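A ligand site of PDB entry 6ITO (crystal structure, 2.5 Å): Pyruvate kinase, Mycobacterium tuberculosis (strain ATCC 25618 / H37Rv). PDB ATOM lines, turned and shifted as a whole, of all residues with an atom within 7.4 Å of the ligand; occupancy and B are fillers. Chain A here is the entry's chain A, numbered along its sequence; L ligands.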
ATOM      1  N   VAL A 235      17.420  26.293 -28.721  1.00  0.00           N
ATOM      2  CA  VAL A 235      16.521  25.221 -28.174  1.00  0.00           C
ATOM      3  C   VAL A 235      15.057  25.559 -28.520  1.00  0.00           C
ATOM      4  O   VAL A 235      14.259  24.610 -28.631  1.00  0.00           O
ATOM      5  CB  VAL A 235      16.716  25.048 -26.649  1.00  0.00           C
ATOM      6  CG1 VAL A 235      15.586  24.228 -26.033  1.00  0.00           C
ATOM      7  CG2 VAL A 235      18.070  24.420 -26.326  1.00  0.00           C
ATOM      8  N   LEU A 236      14.724  26.842 -28.677  1.00  0.00           N
ATOM      9  CA  LEU A 236      13.347  27.311 -28.939  1.00  0.00           C
ATOM     10  C   LEU A 236      13.052  27.279 -30.438  1.00  0.00           C
ATOM     11  O   LEU A 236      11.918  26.951 -30.796  1.00  0.00           O
ATOM     12  CB  LEU A 236      13.148  28.701 -28.363  1.00  0.00           C
ATOM     13  CG  LEU A 236      12.931  28.750 -26.849  1.00  0.00           C
ATOM     14  CD1 LEU A 236      12.947  30.178 -26.331  1.00  0.00           C
ATOM     15  CD2 LEU A 236      11.639  28.054 -26.461  1.00  0.00           C
ATOM     16  N   ALA A 237      14.021  27.604 -31.282  1.00  0.00           N
ATOM     17  CA  ALA A 237      13.867  27.667 -32.761  1.00  0.00           C
ATOM     18  C   ALA A 237      13.941  26.250 -33.356  1.00  0.00           C
ATOM     19  O   ALA A 237      13.259  26.011 -34.338  1.00  0.00           O
ATOM     20  CB  ALA A 237      14.916  28.568 -33.363  1.00  0.00           C
ATOM     21  N   PHE A 238      14.744  25.363 -32.764  1.00  0.00           N
ATOM     22  CA  PHE A 238      14.937  23.962 -33.219  1.00  0.00           C
ATOM     23  C   PHE A 238      13.975  23.049 -32.459  1.00  0.00           C
ATOM     24  O   PHE A 238      13.395  23.513 -31.488  1.00  0.00           O
ATOM     25  CB  PHE A 238      16.394  23.533 -33.049  1.00  0.00           C
ATOM     26  CG  PHE A 238      17.325  24.054 -34.104  1.00  0.00           C
ATOM     27  CD1 PHE A 238      17.901  25.310 -33.989  1.00  0.00           C
ATOM     28  CD2 PHE A 238      17.660  23.283 -35.203  1.00  0.00           C
ATOM     29  CE1 PHE A 238      18.787  25.776 -34.951  1.00  0.00           C
ATOM     30  CE2 PHE A 238      18.546  23.756 -36.154  1.00  0.00           C
ATOM     31  CZ  PHE A 238      19.105  24.997 -36.029  1.00  0.00           C
ATOM     32  N   MET A 267      17.859  22.762 -20.221  1.00  0.00           N
ATOM     33  CA  MET A 267      17.259  23.762 -21.126  1.00  0.00           C
ATOM     34  C   MET A 267      16.263  23.054 -22.090  1.00  0.00           C
ATOM     35  O   MET A 267      15.156  23.585 -22.295  1.00  0.00           O
ATOM     36  CB  MET A 267      18.357  24.459 -21.939  1.00  0.00           C
ATOM     37  CG  MET A 267      17.838  25.589 -22.801  1.00  0.00           C
ATOM     38  SD  MET A 267      17.228  26.934 -21.794  1.00  0.00           S
ATOM     39  CE  MET A 267      18.781  27.728 -21.351  1.00  0.00           C
ATOM     40  N   ALA A 268      16.651  21.909 -22.637  1.00  0.00           N
ATOM     41  CA  ALA A 268      15.803  21.063 -23.478  1.00  0.00           C
ATOM     42  C   ALA A 268      14.524  20.756 -22.728  1.00  0.00           C
ATOM     43  O   ALA A 268      13.464  21.081 -23.249  1.00  0.00           O
ATOM     44  CB  ALA A 268      16.526  19.793 -23.872  1.00  0.00           C
ATOM     45  N   ARG A 269      14.633  20.193 -21.529  1.00  0.00           N
ATOM     46  CA  ARG A 269      13.474  19.673 -20.750  1.00  0.00           C
ATOM     47  C   ARG A 269      12.548  20.827 -20.328  1.00  0.00           C
ATOM     48  O   ARG A 269      11.332  20.607 -20.286  1.00  0.00           O
ATOM     49  CB  ARG A 269      13.950  18.885 -19.519  1.00  0.00           C
ATOM     50  CG  ARG A 269      14.575  17.538 -19.831  1.00  0.00           C
ATOM     51  CD  ARG A 269      15.056  16.842 -18.581  1.00  0.00           C
ATOM     52  NE  ARG A 269      14.028  16.759 -17.563  1.00  0.00           N
ATOM     53  CZ  ARG A 269      14.135  17.236 -16.331  1.00  0.00           C
ATOM     54  NH1 ARG A 269      15.243  17.850 -15.933  1.00  0.00           N
ATOM     55  NH2 ARG A 269      13.126  17.095 -15.486  1.00  0.00           N
ATOM     56  N   GLU A 270      13.091  21.994 -19.995  1.00  0.00           N
ATOM     57  CA  GLU A 270      12.306  23.176 -19.588  1.00  0.00           C
ATOM     58  C   GLU A 270      11.341  23.550 -20.716  1.00  0.00           C
ATOM     59  O   GLU A 270      10.278  24.088 -20.420  1.00  0.00           O
ATOM     60  CB  GLU A 270      13.207  24.359 -19.233  1.00  0.00           C
ATOM     61  CG  GLU A 270      14.054  24.144 -17.986  1.00  0.00           C
ATOM     62  CD  GLU A 270      13.364  24.409 -16.648  1.00  0.00           C
ATOM     63  OE1 GLU A 270      13.998  24.157 -15.599  1.00  0.00           O
ATOM     64  OE2 GLU A 270      12.185  24.873 -16.647  1.00  0.00           O
ATOM     65  N   ASN A 271      11.730  23.301 -21.967  1.00  0.00           N
ATOM     66  CA  ASN A 271      11.017  23.769 -23.187  1.00  0.00           C
ATOM     67  C   ASN A 271      10.416  22.559 -23.926  1.00  0.00           C
ATOM     68  O   ASN A 271       9.870  22.746 -25.081  1.00  0.00           O
ATOM     69  CB  ASN A 271      11.936  24.604 -24.072  1.00  0.00           C
ATOM     70  CG  ASN A 271      12.382  25.870 -23.398  1.00  0.00           C
ATOM     71  OD1 ASN A 271      11.599  26.808 -23.226  1.00  0.00           O
ATOM     72  ND2 ASN A 271      13.640  25.917 -22.989  1.00  0.00           N
ATOM     73  N   ALA A 272      10.449  21.380 -23.274  1.00  0.00           N
ATOM     74  CA  ALA A 272       9.821  20.132 -23.727  1.00  0.00           C
ATOM     75  C   ALA A 272      10.405  19.718 -25.088  1.00  0.00           C
ATOM     76  O   ALA A 272       9.629  19.333 -25.964  1.00  0.00           O
ATOM     77  CB  ALA A 272       8.320  20.315 -23.792  1.00  0.00           C
ATOM     78  N   LYS A 273      11.712  19.839 -25.256  1.00  0.00           N
ATOM     79  CA  LYS A 273      12.414  19.381 -26.482  1.00  0.00           C
ATOM     80  C   LYS A 273      13.282  18.183 -26.139  1.00  0.00           C
ATOM     81  O   LYS A 273      13.848  18.077 -25.040  1.00  0.00           O
ATOM     82  CB  LYS A 273      13.252  20.510 -27.108  1.00  0.00           C
ATOM     83  CG  LYS A 273      12.524  21.830 -27.285  1.00  0.00           C
ATOM     84  CD  LYS A 273      11.477  21.821 -28.349  1.00  0.00           C
ATOM     85  CE  LYS A 273      10.846  23.167 -28.537  1.00  0.00           C
ATOM     86  NZ  LYS A 273      11.626  24.016 -29.473  1.00  0.00           N
ATOM     87  N   LEU A 346      12.203  20.915 -12.711  1.00  0.00           N
ATOM     88  CA  LEU A 346      12.109  22.122 -13.589  1.00  0.00           C
ATOM     89  C   LEU A 346      12.124  23.365 -12.709  1.00  0.00           C
ATOM     90  O   LEU A 346      11.563  23.310 -11.641  1.00  0.00           O
ATOM     91  CB  LEU A 346      10.811  22.055 -14.420  1.00  0.00           C
ATOM     92  CG  LEU A 346      10.621  20.797 -15.250  1.00  0.00           C
ATOM     93  CD1 LEU A 346       9.362  20.909 -16.104  1.00  0.00           C
ATOM     94  CD2 LEU A 346      11.843  20.515 -16.121  1.00  0.00           C
ATOM     95  N   HIS A 348      10.689  26.201 -13.324  1.00  0.00           N
ATOM     96  CA  HIS A 348       9.464  26.994 -13.611  1.00  0.00           C
ATOM     97  C   HIS A 348       8.225  26.101 -13.503  1.00  0.00           C
ATOM     98  O   HIS A 348       8.281  24.903 -13.930  1.00  0.00           O
ATOM     99  CB  HIS A 348       9.620  27.722 -14.976  1.00  0.00           C
ATOM    100  CG  HIS A 348       9.100  26.956 -16.151  1.00  0.00           C
ATOM    101  ND1 HIS A 348       9.707  25.812 -16.620  1.00  0.00           N
ATOM    102  CD2 HIS A 348       8.052  27.199 -16.986  1.00  0.00           C
ATOM    103  CE1 HIS A 348       9.040  25.353 -17.671  1.00  0.00           C
ATOM    104  NE2 HIS A 348       8.028  26.201 -17.910  1.00  0.00           N
ATOM    105  N   ILE A 349       7.155  26.650 -12.934  1.00  0.00           N
ATOM    106  CA  ILE A 349       5.791  26.063 -13.016  1.00  0.00           C
ATOM    107  C   ILE A 349       5.293  26.226 -14.438  1.00  0.00           C
ATOM    108  O   ILE A 349       5.373  27.309 -15.024  1.00  0.00           O
ATOM    109  CB  ILE A 349       4.833  26.696 -11.977  1.00  0.00           C
ATOM    110  CG1 ILE A 349       5.233  26.278 -10.557  1.00  0.00           C
ATOM    111  CG2 ILE A 349       3.387  26.342 -12.281  1.00  0.00           C
ATOM    112  CD1 ILE A 349       5.670  24.803 -10.440  1.00  0.00           C
ATOM    113  N   PRO A 350       4.825  25.124 -15.058  1.00  0.00           N
ATOM    114  CA  PRO A 350       4.296  25.186 -16.420  1.00  0.00           C
ATOM    115  C   PRO A 350       3.224  26.295 -16.570  1.00  0.00           C
ATOM    116  O   PRO A 350       2.461  26.515 -15.604  1.00  0.00           O
ATOM    117  CB  PRO A 350       3.707  23.769 -16.613  1.00  0.00           C
ATOM    118  CG  PRO A 350       4.557  22.878 -15.677  1.00  0.00           C
ATOM    119  CD  PRO A 350       4.829  23.771 -14.491  1.00  0.00           C
ATOM    120  N   ARG A 351       3.203  26.982 -17.732  1.00  0.00           N
ATOM    121  CA  ARG A 351       2.245  28.101 -18.033  1.00  0.00           C
ATOM    122  C   ARG A 351       1.351  27.773 -19.240  1.00  0.00           C
ATOM    123  O   ARG A 351       0.228  28.319 -19.305  1.00  0.00           O
ATOM    124  CB  ARG A 351       3.008  29.403 -18.248  1.00  0.00           C
ATOM    125  CG  ARG A 351       2.427  30.592 -17.479  1.00  0.00           C
ATOM    126  CD  ARG A 351       3.478  31.586 -17.046  1.00  0.00           C
ATOM    127  NE  ARG A 351       4.662  30.901 -16.566  1.00  0.00           N
ATOM    128  CZ  ARG A 351       5.006  30.775 -15.281  1.00  0.00           C
ATOM    129  NH1 ARG A 351       4.276  31.332 -14.332  1.00  0.00           N
ATOM    130  NH2 ARG A 351       6.103  30.095 -14.956  1.00  0.00           N
ATOM    131  N   THR A 352       1.811  26.920 -20.166  1.00  0.00           N
ATOM    132  CA  THR A 352       1.069  26.549 -21.387  1.00  0.00           C
ATOM    133  C   THR A 352       0.054  25.472 -21.037  1.00  0.00           C
ATOM    134  O   THR A 352       0.367  24.617 -20.160  1.00  0.00           O
ATOM    135  CB  THR A 352       1.976  26.093 -22.535  1.00  0.00           C
ATOM    136  OG1 THR A 352       2.311  24.718 -22.356  1.00  0.00           O
ATOM    137  CG2 THR A 352       3.248  26.908 -22.647  1.00  0.00           C
ATOM    138  N   LYS A 353      -1.100  25.507 -21.696  1.00  0.00           N
ATOM    139  CA  LYS A 353      -2.239  24.599 -21.429  1.00  0.00           C
ATOM    140  C   LYS A 353      -1.736  23.165 -21.405  1.00  0.00           C
ATOM    141  O   LYS A 353      -2.114  22.429 -20.507  1.00  0.00           O
ATOM    142  CB  LYS A 353      -3.318  24.776 -22.503  1.00  0.00           C
ATOM    143  CG  LYS A 353      -4.623  24.067 -22.221  1.00  0.00           C
ATOM    144  CD  LYS A 353      -5.732  24.402 -23.214  1.00  0.00           C
ATOM    145  CE  LYS A 353      -5.701  23.530 -24.444  1.00  0.00           C
ATOM    146  NZ  LYS A 353      -6.580  24.072 -25.502  1.00  0.00           N
ATOM    147  N   ARG A 354      -0.887  22.803 -22.350  1.00  0.00           N
ATOM    148  CA  ARG A 354      -0.445  21.397 -22.552  1.00  0.00           C
ATOM    149  C   ARG A 354       0.522  20.987 -21.444  1.00  0.00           C
ATOM    150  O   ARG A 354       0.436  19.833 -20.980  1.00  0.00           O
ATOM    151  CB  ARG A 354       0.154  21.244 -23.943  1.00  0.00           C
ATOM    152  CG  ARG A 354      -0.884  21.240 -25.036  1.00  0.00           C
ATOM    153  CD  ARG A 354      -0.289  21.114 -26.401  1.00  0.00           C
ATOM    154  NE  ARG A 354       0.253  22.358 -26.891  1.00  0.00           N
ATOM    155  CZ  ARG A 354       0.788  22.503 -28.092  1.00  0.00           C
ATOM    156  NH1 ARG A 354       0.829  21.479 -28.923  1.00  0.00           N
ATOM    157  NH2 ARG A 354       1.280  23.666 -28.475  1.00  0.00           N
ATOM    158  N   GLY A 355       1.406  21.898 -21.020  1.00  0.00           N
ATOM    159  CA  GLY A 355       2.314  21.692 -19.880  1.00  0.00           C
ATOM    160  C   GLY A 355       1.550  21.453 -18.580  1.00  0.00           C
ATOM    161  O   GLY A 355       1.810  20.422 -17.918  1.00  0.00           O
ATOM    162  N   VAL A 356       0.644  22.368 -18.241  1.00  0.00           N
ATOM    163  CA  VAL A 356      -0.162  22.331 -17.008  1.00  0.00           C
ATOM    164  C   VAL A 356      -0.924  21.008 -16.928  1.00  0.00           C
ATOM    165  O   VAL A 356      -0.939  20.410 -15.841  1.00  0.00           O
ATOM    166  CB  VAL A 356      -1.132  23.505 -16.940  1.00  0.00           C
ATOM    167  CG1 VAL A 356      -2.230  23.263 -15.932  1.00  0.00           C
ATOM    168  CG2 VAL A 356      -0.405  24.805 -16.652  1.00  0.00           C
ATOM    169  N   SER A 358      -0.505  18.062 -18.672  1.00  0.00           N
ATOM    170  CA  SER A 358       0.395  16.868 -18.652  1.00  0.00           C
ATOM    171  C   SER A 358       1.013  16.734 -17.269  1.00  0.00           C
ATOM    172  O   SER A 358       1.137  15.604 -16.789  1.00  0.00           O
ATOM    173  CB  SER A 358       1.439  16.955 -19.738  1.00  0.00           C
ATOM    174  OG  SER A 358       2.039  18.252 -19.745  1.00  0.00           O
ATOM    175  N   ASP A 381       3.679  17.030 -29.043  1.00  0.00           N
ATOM    176  CA  ASP A 381       3.947  18.110 -28.056  1.00  0.00           C
ATOM    177  C   ASP A 381       3.396  17.725 -26.690  1.00  0.00           C
ATOM    178  O   ASP A 381       4.141  17.794 -25.743  1.00  0.00           O
ATOM    179  CB  ASP A 381       3.352  19.462 -28.462  1.00  0.00           C
ATOM    180  CG  ASP A 381       3.674  20.572 -27.471  1.00  0.00           C
ATOM    181  OD1 ASP A 381       2.978  20.668 -26.419  1.00  0.00           O
ATOM    182  OD2 ASP A 381       4.676  21.315 -27.716  1.00  0.00           O
ATOM    183  N   ARG A 385       5.682  17.019 -23.042  1.00  0.00           N
ATOM    184  CA  ARG A 385       5.545  17.807 -21.782  1.00  0.00           C
ATOM    185  C   ARG A 385       5.316  16.862 -20.606  1.00  0.00           C
ATOM    186  O   ARG A 385       5.602  17.273 -19.458  1.00  0.00           O
ATOM    187  CB  ARG A 385       4.433  18.837 -21.917  1.00  0.00           C
ATOM    188  CG  ARG A 385       4.552  19.687 -23.164  1.00  0.00           C
ATOM    189  CD  ARG A 385       4.001  21.067 -23.016  1.00  0.00           C
ATOM    190  NE  ARG A 385       4.186  21.776 -24.266  1.00  0.00           N
ATOM    191  CZ  ARG A 385       5.073  22.738 -24.469  1.00  0.00           C
ATOM    192  NH1 ARG A 385       5.836  23.156 -23.481  1.00  0.00           N
ATOM    193  NH2 ARG A 385       5.191  23.278 -25.666  1.00  0.00           N
ATOM    194  N   ARG A 388       9.309  14.774 -20.218  1.00  0.00           N
ATOM    195  CA  ARG A 388      10.358  15.593 -19.568  1.00  0.00           C
ATOM    196  C   ARG A 388      10.252  15.465 -18.046  1.00  0.00           C
ATOM    197  O   ARG A 388      11.228  15.740 -17.404  1.00  0.00           O
ATOM    198  CB  ARG A 388      10.222  17.051 -20.010  1.00  0.00           C
ATOM    199  CG  ARG A 388       8.963  17.724 -19.479  1.00  0.00           C
ATOM    200  CD  ARG A 388       8.883  19.194 -19.849  1.00  0.00           C
ATOM    201  NE  ARG A 388       7.588  19.772 -19.507  1.00  0.00           N
ATOM    202  CZ  ARG A 388       7.316  21.069 -19.504  1.00  0.00           C
ATOM    203  NH1 ARG A 388       8.251  21.936 -19.835  1.00  0.00           N
ATOM    204  NH2 ARG A 388       6.100  21.483 -19.201  1.00  0.00           N
HETATM  205  C1  LIG L   1       7.734  26.772 -26.879  1.00  0.00           C
HETATM  206  O1  LIG L   1       8.141  26.192 -27.873  1.00  0.00           O
HETATM  207  C2  LIG L   1       8.217  26.382 -25.488  1.00  0.00           C
HETATM  208  O2  LIG L   1       8.442  25.003 -25.482  1.00  0.00           O
HETATM  209  C3  LIG L   1       7.189  26.896 -24.352  1.00  0.00           C
HETATM  210  O3  LIG L   1       6.798  28.201 -24.626  1.00  0.00           O
HETATM  211  C4  LIG L   1       7.842  26.705 -22.938  1.00  0.00           C
HETATM  212  O4  LIG L   1       8.404  25.436 -22.955  1.00  0.00           O
HETATM  213  C5  LIG L   1       6.827  26.848 -21.791  1.00  0.00           C
HETATM  214  O5  LIG L   1       6.165  25.674 -21.729  1.00  0.00           O
HETATM  215  P1  LIG L   1       5.563  25.022 -20.115  1.00  0.00           P
HETATM  216  O6  LIG L   1       6.833  24.473 -19.522  1.00  0.00           O
HETATM  217  O7  LIG L   1       4.555  24.019 -20.610  1.00  0.00           O
HETATM  218  O8  LIG L   1       5.007  26.309 -19.510  1.00  0.00           O
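O of Asn 271 lies within hydrogen-bond range of O2 of the ligand (2.7 Å).
OD1 of Asn 271 lies close to O4 of the ligand.
OG1 of Thr 352 sits at hydrogen-bond distance from O7 of the ligand (2.9 Å).
The guanidinium group (NH1) of Arg 388 lies within salt-bridge range of an oxygen (O6) of the ligand (2.9 Å).
The backbone carbonyl oxygen (O) of Glu 270 lies within hydrogen-bond range of an oxygen (O4) of the ligand (3.4 Å).
The guanidinium group (NH1) of Arg 385 is in salt-bridge range of an oxygen (O7) of the ligand (3.3 Å).
The backbone NH (N) of Arg 351 sits at hydrogen-bond distance from an oxygen (O8) of the ligand, at 2.6 Å.
A ring nitrogen (NE2) of His 348 sits at hydrogen-bond distance from an oxygen (O6) of the ligand (2.6 Å).
The backbone NH of Thr 352 is in hydrogen-bond range of an oxygen (O8) of the ligand, at 3.3 Å.
NE of Arg 385 is in salt-bridge range of OD1 of Asp 381 (2.7 Å).
The side-chain hydroxyl (OG) of Ser 358 sits at hydrogen-bond distance from the backbone carbonyl oxygen (O) of Gly 355, 2.8 Å away.
The guanidinium group (NH2) of Arg 351 sits at hydrogen-bond distance from the backbone carbonyl oxygen (O) of Ile 349.
The backbone carbonyl oxygen of Glu 270 is in hydrogen-bond range of the guanidinium group of Arg 388 (3.0 Å).
A ring nitrogen (ND1) of His 348 sits at hydrogen-bond distance from the side-chain carboxylate (OE2) of Glu 270.
The side-chain hydroxyl of Thr 352 sits at hydrogen-bond distance from the backbone NH of Gly 355 (3.2 Å).
The guanidinium group (NE) of Arg 388 is in hydrogen-bond range of the backbone carbonyl oxygen (O) of Arg 385, at 3.2 Å.
The backbone carbonyl oxygen of Arg 388 lies within hydrogen-bond range of the guanidinium group of Arg 269 (3.0 Å).
CD2 of Leu 236 touches C2 of the ligand, at 3.9 Å.
CA of Pro 350 touches O8 of the ligand (3.4 Å).
Gly 355 touches the ligand.
Of the 25 residues printed, 10 come within 4 Å of the ligand.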
